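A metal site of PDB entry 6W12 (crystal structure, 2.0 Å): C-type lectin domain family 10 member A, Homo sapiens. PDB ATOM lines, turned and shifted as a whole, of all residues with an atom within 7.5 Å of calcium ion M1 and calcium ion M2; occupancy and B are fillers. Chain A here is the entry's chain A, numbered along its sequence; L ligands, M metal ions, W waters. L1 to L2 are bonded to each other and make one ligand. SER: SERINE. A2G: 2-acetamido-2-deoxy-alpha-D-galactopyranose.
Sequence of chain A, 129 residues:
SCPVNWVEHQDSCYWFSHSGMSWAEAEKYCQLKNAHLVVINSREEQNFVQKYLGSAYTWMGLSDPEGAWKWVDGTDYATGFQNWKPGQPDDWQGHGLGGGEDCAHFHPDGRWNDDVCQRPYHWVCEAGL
Within 4 Å of calcium ion M2: Gln 88, Asp 90, Glu 101, Asn 113 and Asp 114.
Along chain A the residues within 4 Å of calcium ion M2 span positions 88 to 114.
OD2 of Asp 114 is in hydrogen-bond range of N of Asp 91, at 2.7 Å.
N of Trp 92 lies close to OE1 of Glu 101 (3.2 Å).
The backbone NH of Asp 102 lies within hydrogen-bond range of the backbone carbonyl oxygen of Asp 115, 3.2 Å away.
The backbone NH (N) of His 105 lies within hydrogen-bond range of the backbone carbonyl oxygen (O) of Asn 113, 2.9 Å away.
The side-chain carboxylate of Asp 90 lies close to the backbone NH of Trp 92, at 3.4 Å.
Calcium ion M1 is bound by water W2 (2.3 Å), OD1 of Asp 91 (2.3 Å), O of Glu 101 (2.4 Å), OD1 of Asp 102 (2.4 Å), water W1 (2.5 Å), OD1 of Asp 64 (2.7 Å) and OD2 of Asp 64 (2.7 Å).
Calcium ion M1 has seven donor atoms within binding distance.
Within 4 Å of calcium ion M1: Asp 64, Asp 91, Glu 101 and Asp 102.
The nearest printed residue that does not touch calcium ion M1 is Asp 114 (4.6 Å).
Calcium ion M2 is bound by the side-chain carboxylate of Asp 114, the side-chain carboxylate of Glu 101, the backbone carbonyl oxygen of Asp 114, the side-chain amide oxygen of Asn 113, the side-chain carboxylate of Asp 90, the side-chain amide oxygen of Gln 88, an oxygen (O4) of A2G L2 and an oxygen (O3) of A2G L2.
Calcium ion M2 has eight donor atoms within binding distance.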
ATOM      1  N   SER A  63     -20.465  23.461  28.426  1.00  0.00           N
ATOM      2  CA  SER A  63     -21.013  22.772  27.248  1.00  0.00           C
ATOM      3  C   SER A  63     -20.565  23.476  25.970  1.00  0.00           C
ATOM      4  O   SER A  63     -20.159  24.650  26.053  1.00  0.00           O
ATOM      5  CB  SER A  63     -22.524  22.672  27.331  1.00  0.00           C
ATOM      6  OG  SER A  63     -23.107  23.971  27.271  1.00  0.00           O
ATOM      7  N   ASP A  64     -20.643  22.783  24.825  1.00  0.00           N
ATOM      8  CA  ASP A  64     -20.270  23.385  23.511  1.00  0.00           C
ATOM      9  C   ASP A  64     -21.238  22.997  22.386  1.00  0.00           C
ATOM     10  O   ASP A  64     -20.814  22.683  21.288  1.00  0.00           O
ATOM     11  CB  ASP A  64     -18.846  23.007  23.129  1.00  0.00           C
ATOM     12  CG  ASP A  64     -18.672  21.574  22.687  1.00  0.00           C
ATOM     13  OD1 ASP A  64     -19.527  20.740  23.037  1.00  0.00           O
ATOM     14  OD2 ASP A  64     -17.698  21.288  21.942  1.00  0.00           O
ATOM     15  N   PRO A  65     -22.560  23.032  22.587  1.00  0.00           N
ATOM     16  CA  PRO A  65     -23.481  22.558  21.550  1.00  0.00           C
ATOM     17  C   PRO A  65     -23.483  23.455  20.295  1.00  0.00           C
ATOM     18  O   PRO A  65     -23.617  22.915  19.215  1.00  0.00           O
ATOM     19  CB  PRO A  65     -24.833  22.594  22.263  1.00  0.00           C
ATOM     20  CG  PRO A  65     -24.668  23.714  23.278  1.00  0.00           C
ATOM     21  CD  PRO A  65     -23.255  23.541  23.782  1.00  0.00           C
ATOM     22  N   GLY A  67     -20.913  25.102  19.251  1.00  0.00           N
ATOM     23  CA  GLY A  67     -19.611  24.839  18.606  1.00  0.00           C
ATOM     24  C   GLY A  67     -18.408  25.255  19.458  1.00  0.00           C
ATOM     25  O   GLY A  67     -17.327  24.669  19.235  1.00  0.00           O
ATOM     26  N   ALA A  68     -18.536  26.216  20.388  1.00  0.00           N
ATOM     27  CA  ALA A  68     -17.437  26.651  21.293  1.00  0.00           C
ATOM     28  C   ALA A  68     -17.811  26.341  22.745  1.00  0.00           C
ATOM     29  O   ALA A  68     -18.994  26.387  23.052  1.00  0.00           O
ATOM     30  CB  ALA A  68     -17.154  28.109  21.086  1.00  0.00           C
ATOM     31  N   TRP A  69     -16.839  26.041  23.604  1.00  0.00           N
ATOM     32  CA  TRP A  69     -17.070  25.727  25.051  1.00  0.00           C
ATOM     33  C   TRP A  69     -17.534  26.986  25.763  1.00  0.00           C
ATOM     34  O   TRP A  69     -16.905  28.015  25.620  1.00  0.00           O
ATOM     35  CB  TRP A  69     -15.831  25.140  25.719  1.00  0.00           C
ATOM     36  CG  TRP A  69     -15.630  23.737  25.252  1.00  0.00           C
ATOM     37  CD1 TRP A  69     -14.800  23.284  24.265  1.00  0.00           C
ATOM     38  CD2 TRP A  69     -16.367  22.600  25.720  1.00  0.00           C
ATOM     39  NE1 TRP A  69     -14.966  21.936  24.099  1.00  0.00           N
ATOM     40  CE2 TRP A  69     -15.905  21.477  24.989  1.00  0.00           C
ATOM     41  CE3 TRP A  69     -17.344  22.418  26.690  1.00  0.00           C
ATOM     42  CZ2 TRP A  69     -16.427  20.212  25.188  1.00  0.00           C
ATOM     43  CZ3 TRP A  69     -17.855  21.156  26.880  1.00  0.00           C
ATOM     44  CH2 TRP A  69     -17.405  20.071  26.138  1.00  0.00           C
ATOM     45  N   TRP A  84      -9.025  19.209  31.972  1.00  0.00           N
ATOM     46  CA  TRP A  84      -9.434  18.042  31.135  1.00  0.00           C
ATOM     47  C   TRP A  84      -8.582  16.817  31.459  1.00  0.00           C
ATOM     48  O   TRP A  84      -7.335  16.980  31.746  1.00  0.00           O
ATOM     49  CB  TRP A  84      -9.311  18.348  29.649  1.00  0.00           C
ATOM     50  CG  TRP A  84     -10.222  19.453  29.232  1.00  0.00           C
ATOM     51  CD1 TRP A  84      -9.858  20.736  28.985  1.00  0.00           C
ATOM     52  CD2 TRP A  84     -11.630  19.375  29.009  1.00  0.00           C
ATOM     53  NE1 TRP A  84     -10.948  21.463  28.630  1.00  0.00           N
ATOM     54  CE2 TRP A  84     -12.043  20.667  28.633  1.00  0.00           C
ATOM     55  CE3 TRP A  84     -12.584  18.356  29.084  1.00  0.00           C
ATOM     56  CZ2 TRP A  84     -13.353  20.969  28.313  1.00  0.00           C
ATOM     57  CZ3 TRP A  84     -13.896  18.670  28.814  1.00  0.00           C
ATOM     58  CH2 TRP A  84     -14.267  19.953  28.395  1.00  0.00           C
ATOM     59  N   GLY A  87      -6.398  13.715  26.541  1.00  0.00           N
ATOM     60  CA  GLY A  87      -7.077  13.306  25.294  1.00  0.00           C
ATOM     61  C   GLY A  87      -8.494  13.858  25.243  1.00  0.00           C
ATOM     62  O   GLY A  87      -9.176  13.555  24.272  1.00  0.00           O
ATOM     63  N   GLN A  88      -8.914  14.626  26.259  1.00  0.00           N
ATOM     64  CA  GLN A  88     -10.248  15.283  26.256  1.00  0.00           C
ATOM     65  C   GLN A  88     -10.014  16.779  26.121  1.00  0.00           C
ATOM     66  O   GLN A  88      -8.947  17.295  26.464  1.00  0.00           O
ATOM     67  CB  GLN A  88     -11.040  14.892  27.499  1.00  0.00           C
ATOM     68  CG  GLN A  88     -11.052  13.382  27.744  1.00  0.00           C
ATOM     69  CD  GLN A  88     -11.833  12.608  26.706  1.00  0.00           C
ATOM     70  OE1 GLN A  88     -12.564  13.175  25.894  1.00  0.00           O
ATOM     71  NE2 GLN A  88     -11.682  11.292  26.689  1.00  0.00           N
ATOM     72  N   PRO A  89     -10.977  17.543  25.597  1.00  0.00           N
ATOM     73  CA  PRO A  89     -12.224  17.009  25.039  1.00  0.00           C
ATOM     74  C   PRO A  89     -11.953  16.437  23.634  1.00  0.00           C
ATOM     75  O   PRO A  89     -11.056  16.903  23.011  1.00  0.00           O
ATOM     76  CB  PRO A  89     -13.110  18.233  24.953  1.00  0.00           C
ATOM     77  CG  PRO A  89     -12.165  19.380  24.737  1.00  0.00           C
ATOM     78  CD  PRO A  89     -10.893  18.999  25.476  1.00  0.00           C
ATOM     79  N   ASP A  90     -12.722  15.438  23.194  1.00  0.00           N
ATOM     80  CA  ASP A  90     -12.495  14.750  21.902  1.00  0.00           C
ATOM     81  C   ASP A  90     -13.759  14.779  21.046  1.00  0.00           C
ATOM     82  O   ASP A  90     -13.669  14.326  19.926  1.00  0.00           O
ATOM     83  CB  ASP A  90     -11.955  13.337  22.125  1.00  0.00           C
ATOM     84  CG  ASP A  90     -12.885  12.431  22.897  1.00  0.00           C
ATOM     85  OD1 ASP A  90     -13.953  12.948  23.355  1.00  0.00           O
ATOM     86  OD2 ASP A  90     -12.595  11.211  22.988  1.00  0.00           O
ATOM     87  N   ASP A  91     -14.914  15.246  21.549  1.00  0.00           N
ATOM     88  CA  ASP A  91     -16.186  15.286  20.773  1.00  0.00           C
ATOM     89  C   ASP A  91     -16.454  13.882  20.161  1.00  0.00           C
ATOM     90  O   ASP A  91     -16.835  13.813  18.974  1.00  0.00           O
ATOM     91  CB  ASP A  91     -16.153  16.363  19.681  1.00  0.00           C
ATOM     92  CG  ASP A  91     -17.526  16.771  19.148  1.00  0.00           C
ATOM     93  OD1 ASP A  91     -18.467  16.956  19.968  1.00  0.00           O
ATOM     94  OD2 ASP A  91     -17.647  16.982  17.941  1.00  0.00           O
ATOM     95  N   TRP A  92     -16.278  12.812  20.925  1.00  0.00           N
ATOM     96  CA  TRP A  92     -16.297  11.415  20.408  1.00  0.00           C
ATOM     97  C   TRP A  92     -17.665  11.100  19.792  1.00  0.00           C
ATOM     98  O   TRP A  92     -18.681  11.473  20.420  1.00  0.00           O
ATOM     99  CB  TRP A  92     -15.986  10.449  21.524  1.00  0.00           C
ATOM    100  CG  TRP A  92     -15.785   9.029  21.148  1.00  0.00           C
ATOM    101  CD1 TRP A  92     -14.951   8.515  20.201  1.00  0.00           C
ATOM    102  CD2 TRP A  92     -16.351   7.907  21.829  1.00  0.00           C
ATOM    103  NE1 TRP A  92     -14.985   7.147  20.231  1.00  0.00           N
ATOM    104  CE2 TRP A  92     -15.846   6.752  21.217  1.00  0.00           C
ATOM    105  CE3 TRP A  92     -17.252   7.788  22.905  1.00  0.00           C
ATOM    106  CZ2 TRP A  92     -16.195   5.483  21.650  1.00  0.00           C
ATOM    107  CZ3 TRP A  92     -17.584   6.536  23.331  1.00  0.00           C
ATOM    108  CH2 TRP A  92     -17.090   5.397  22.687  1.00  0.00           C
ATOM    109  N   GLY A 100     -21.613  14.180  18.511  1.00  0.00           N
ATOM    110  CA  GLY A 100     -20.362  14.025  19.271  1.00  0.00           C
ATOM    111  C   GLY A 100     -20.640  14.068  20.746  1.00  0.00           C
ATOM    112  O   GLY A 100     -21.512  13.358  21.176  1.00  0.00           O
ATOM    113  N   GLU A 101     -19.975  14.927  21.490  1.00  0.00           N
ATOM    114  CA  GLU A 101     -20.128  14.982  22.967  1.00  0.00           C
ATOM    115  C   GLU A 101     -20.098  16.451  23.345  1.00  0.00           C
ATOM    116  O   GLU A 101     -19.103  17.113  23.037  1.00  0.00           O
ATOM    117  CB  GLU A 101     -18.981  14.225  23.647  1.00  0.00           C
ATOM    118  CG  GLU A 101     -19.090  12.707  23.498  1.00  0.00           C
ATOM    119  CD  GLU A 101     -17.945  11.948  24.137  1.00  0.00           C
ATOM    120  OE1 GLU A 101     -16.812  12.446  24.044  1.00  0.00           O
ATOM    121  OE2 GLU A 101     -18.205  10.889  24.792  1.00  0.00           O
ATOM    122  N   ASP A 102     -21.140  16.994  23.961  1.00  0.00           N
ATOM    123  CA  ASP A 102     -21.214  18.468  24.076  1.00  0.00           C
ATOM    124  C   ASP A 102     -21.331  18.916  25.526  1.00  0.00           C
ATOM    125  O   ASP A 102     -21.459  20.109  25.718  1.00  0.00           O
ATOM    126  CB  ASP A 102     -22.356  19.018  23.241  1.00  0.00           C
ATOM    127  CG  ASP A 102     -22.214  18.768  21.738  1.00  0.00           C
ATOM    128  OD1 ASP A 102     -21.047  18.497  21.261  1.00  0.00           O
ATOM    129  OD2 ASP A 102     -23.236  18.773  21.078  1.00  0.00           O
ATOM    130  N   CYS A 103     -21.199  18.062  26.520  1.00  0.00           N
ATOM    131  CA  CYS A 103     -21.380  18.465  27.938  1.00  0.00           C
ATOM    132  C   CYS A 103     -20.197  17.951  28.770  1.00  0.00           C
ATOM    133  O   CYS A 103     -19.823  16.768  28.572  1.00  0.00           O
ATOM    134  CB  CYS A 103     -22.685  17.907  28.496  1.00  0.00           C
ATOM    135  SG  CYS A 103     -24.190  18.665  27.824  1.00  0.00           S
ATOM    136  N   HIS A 105     -18.265  16.769  32.315  1.00  0.00           N
ATOM    137  CA  HIS A 105     -18.464  16.230  33.672  1.00  0.00           C
ATOM    138  C   HIS A 105     -17.136  15.949  34.321  1.00  0.00           C
ATOM    139  O   HIS A 105     -16.112  15.776  33.608  1.00  0.00           O
ATOM    140  CB  HIS A 105     -19.331  14.961  33.646  1.00  0.00           C
ATOM    141  CG  HIS A 105     -18.658  13.820  32.974  1.00  0.00           C
ATOM    142  ND1 HIS A 105     -17.945  12.871  33.694  1.00  0.00           N
ATOM    143  CD2 HIS A 105     -18.556  13.490  31.665  1.00  0.00           C
ATOM    144  CE1 HIS A 105     -17.453  11.966  32.841  1.00  0.00           C
ATOM    145  NE2 HIS A 105     -17.791  12.332  31.578  1.00  0.00           N
ATOM    146  N   TRP A 112     -11.738  16.373  33.873  1.00  0.00           N
ATOM    147  CA  TRP A 112     -12.978  16.604  33.076  1.00  0.00           C
ATOM    148  C   TRP A 112     -13.011  15.752  31.815  1.00  0.00           C
ATOM    149  O   TRP A 112     -11.952  15.491  31.207  1.00  0.00           O
ATOM    150  CB  TRP A 112     -13.130  18.049  32.679  1.00  0.00           C
ATOM    151  CG  TRP A 112     -12.970  19.014  33.792  1.00  0.00           C
ATOM    152  CD1 TRP A 112     -12.991  18.769  35.135  1.00  0.00           C
ATOM    153  CD2 TRP A 112     -12.903  20.441  33.647  1.00  0.00           C
ATOM    154  NE1 TRP A 112     -12.861  19.948  35.820  1.00  0.00           N
ATOM    155  CE2 TRP A 112     -12.829  20.980  34.940  1.00  0.00           C
ATOM    156  CE3 TRP A 112     -12.878  21.302  32.549  1.00  0.00           C
ATOM    157  CZ2 TRP A 112     -12.719  22.342  35.147  1.00  0.00           C
ATOM    158  CZ3 TRP A 112     -12.788  22.657  32.763  1.00  0.00           C
ATOM    159  CH2 TRP A 112     -12.693  23.172  34.049  1.00  0.00           C
ATOM    160  N   ASN A 113     -14.230  15.444  31.368  1.00  0.00           N
ATOM    161  CA  ASN A 113     -14.499  14.752  30.088  1.00  0.00           C
ATOM    162  C   ASN A 113     -15.714  15.412  29.435  1.00  0.00           C
ATOM    163  O   ASN A 113     -16.632  15.823  30.162  1.00  0.00           O
ATOM    164  CB  ASN A 113     -14.712  13.255  30.287  1.00  0.00           C
ATOM    165  CG  ASN A 113     -15.184  12.578  29.021  1.00  0.00           C
ATOM    166  OD1 ASN A 113     -14.505  12.654  28.006  1.00  0.00           O
ATOM    167  ND2 ASN A 113     -16.345  11.941  29.066  1.00  0.00           N
ATOM    168  N   ASP A 114     -15.719  15.479  28.115  1.00  0.00           N
ATOM    169  CA  ASP A 114     -16.914  15.768  27.316  1.00  0.00           C
ATOM    170  C   ASP A 114     -17.695  14.476  27.042  1.00  0.00           C
ATOM    171  O   ASP A 114     -17.093  13.491  26.624  1.00  0.00           O
ATOM    172  CB  ASP A 114     -16.566  16.555  26.072  1.00  0.00           C
ATOM    173  CG  ASP A 114     -15.629  15.895  25.080  1.00  0.00           C
ATOM    174  OD1 ASP A 114     -14.876  14.958  25.503  1.00  0.00           O
ATOM    175  OD2 ASP A 114     -15.699  16.294  23.876  1.00  0.00           O
ATOM    176  N   ASP A 115     -19.026  14.475  27.240  1.00  0.00           N
ATOM    177  CA  ASP A 115     -19.827  13.244  27.075  1.00  0.00           C
ATOM    178  C   ASP A 115     -21.166  13.651  26.476  1.00  0.00           C
ATOM    179  O   ASP A 115     -21.421  14.848  26.300  1.00  0.00           O
ATOM    180  CB  ASP A 115     -20.018  12.538  28.420  1.00  0.00           C
ATOM    181  CG  ASP A 115     -20.076  11.019  28.351  1.00  0.00           C
ATOM    182  OD1 ASP A 115     -20.716  10.511  27.435  1.00  0.00           O
ATOM    183  OD2 ASP A 115     -19.491  10.331  29.256  1.00  0.00           O
ATOM    184  N   VAL A 116     -22.009  12.657  26.257  1.00  0.00           N
ATOM    185  CA  VAL A 116     -23.341  12.833  25.656  1.00  0.00           C
ATOM    186  C   VAL A 116     -24.204  13.522  26.712  1.00  0.00           C
ATOM    187  O   VAL A 116     -24.368  12.984  27.821  1.00  0.00           O
ATOM    188  CB  VAL A 116     -23.875  11.460  25.200  1.00  0.00           C
ATOM    189  CG1 VAL A 116     -25.338  11.516  24.837  1.00  0.00           C
ATOM    190  CG2 VAL A 116     -23.005  10.928  24.035  1.00  0.00           C
HETATM  191  N   SER L   1     -15.506   4.048  26.167  1.00  0.00           N
HETATM  192  CA  SER L   1     -16.331   4.416  27.347  1.00  0.00           C
HETATM  193  C   SER L   1     -17.820   4.219  26.976  1.00  0.00           C
HETATM  194  O   SER L   1     -18.400   3.118  27.055  1.00  0.00           O
HETATM  195  CB  SER L   1     -15.855   5.791  27.823  1.00  0.00           C
HETATM  196  OG  SER L   1     -15.047   6.432  26.821  1.00  0.00           O
HETATM  197  OXT SER L   1     -18.545   5.113  26.547  1.00  0.00           O
HETATM  198  O5  A2G L   2     -13.271   7.701  26.136  1.00  0.00           O
HETATM  199  C1  A2G L   2     -14.180   7.484  27.209  1.00  0.00           C
HETATM  200  C2  A2G L   2     -14.925   8.814  27.445  1.00  0.00           C
HETATM  201  N2  A2G L   2     -15.823   8.773  28.584  1.00  0.00           N
HETATM  202  C3  A2G L   2     -15.669   9.283  26.192  1.00  0.00           C
HETATM  203  O3  A2G L   2     -16.255  10.559  26.365  1.00  0.00           O
HETATM  204  C4  A2G L   2     -14.728   9.325  24.990  1.00  0.00           C
HETATM  205  O4  A2G L   2     -13.895  10.481  25.130  1.00  0.00           O
HETATM  206  C5  A2G L   2     -13.942   8.016  24.904  1.00  0.00           C
HETATM  207  C6  A2G L   2     -12.898   8.046  23.811  1.00  0.00           C
HETATM  208  O6  A2G L   2     -12.531   6.736  23.426  1.00  0.00           O
HETATM  209  C7  A2G L   2     -15.453   9.044  29.844  1.00  0.00           C
HETATM  210  O7  A2G L   2     -14.374   9.570  30.108  1.00  0.00           O
HETATM  211  C8  A2G L   2     -16.448   8.711  30.910  1.00  0.00           C
HETATM  212 CA    CA M   1     -18.647  18.811  21.372  1.00  0.00          CA
HETATM  213 CA    CA M   2     -15.004  12.701  25.601  1.00  0.00          CA
HETATM  214  O   HOH W   1     -19.287  20.318  19.537  1.00  0.00           O
HETATM  215  O   HOH W   2     -16.566  18.389  22.244  1.00  0.00           O
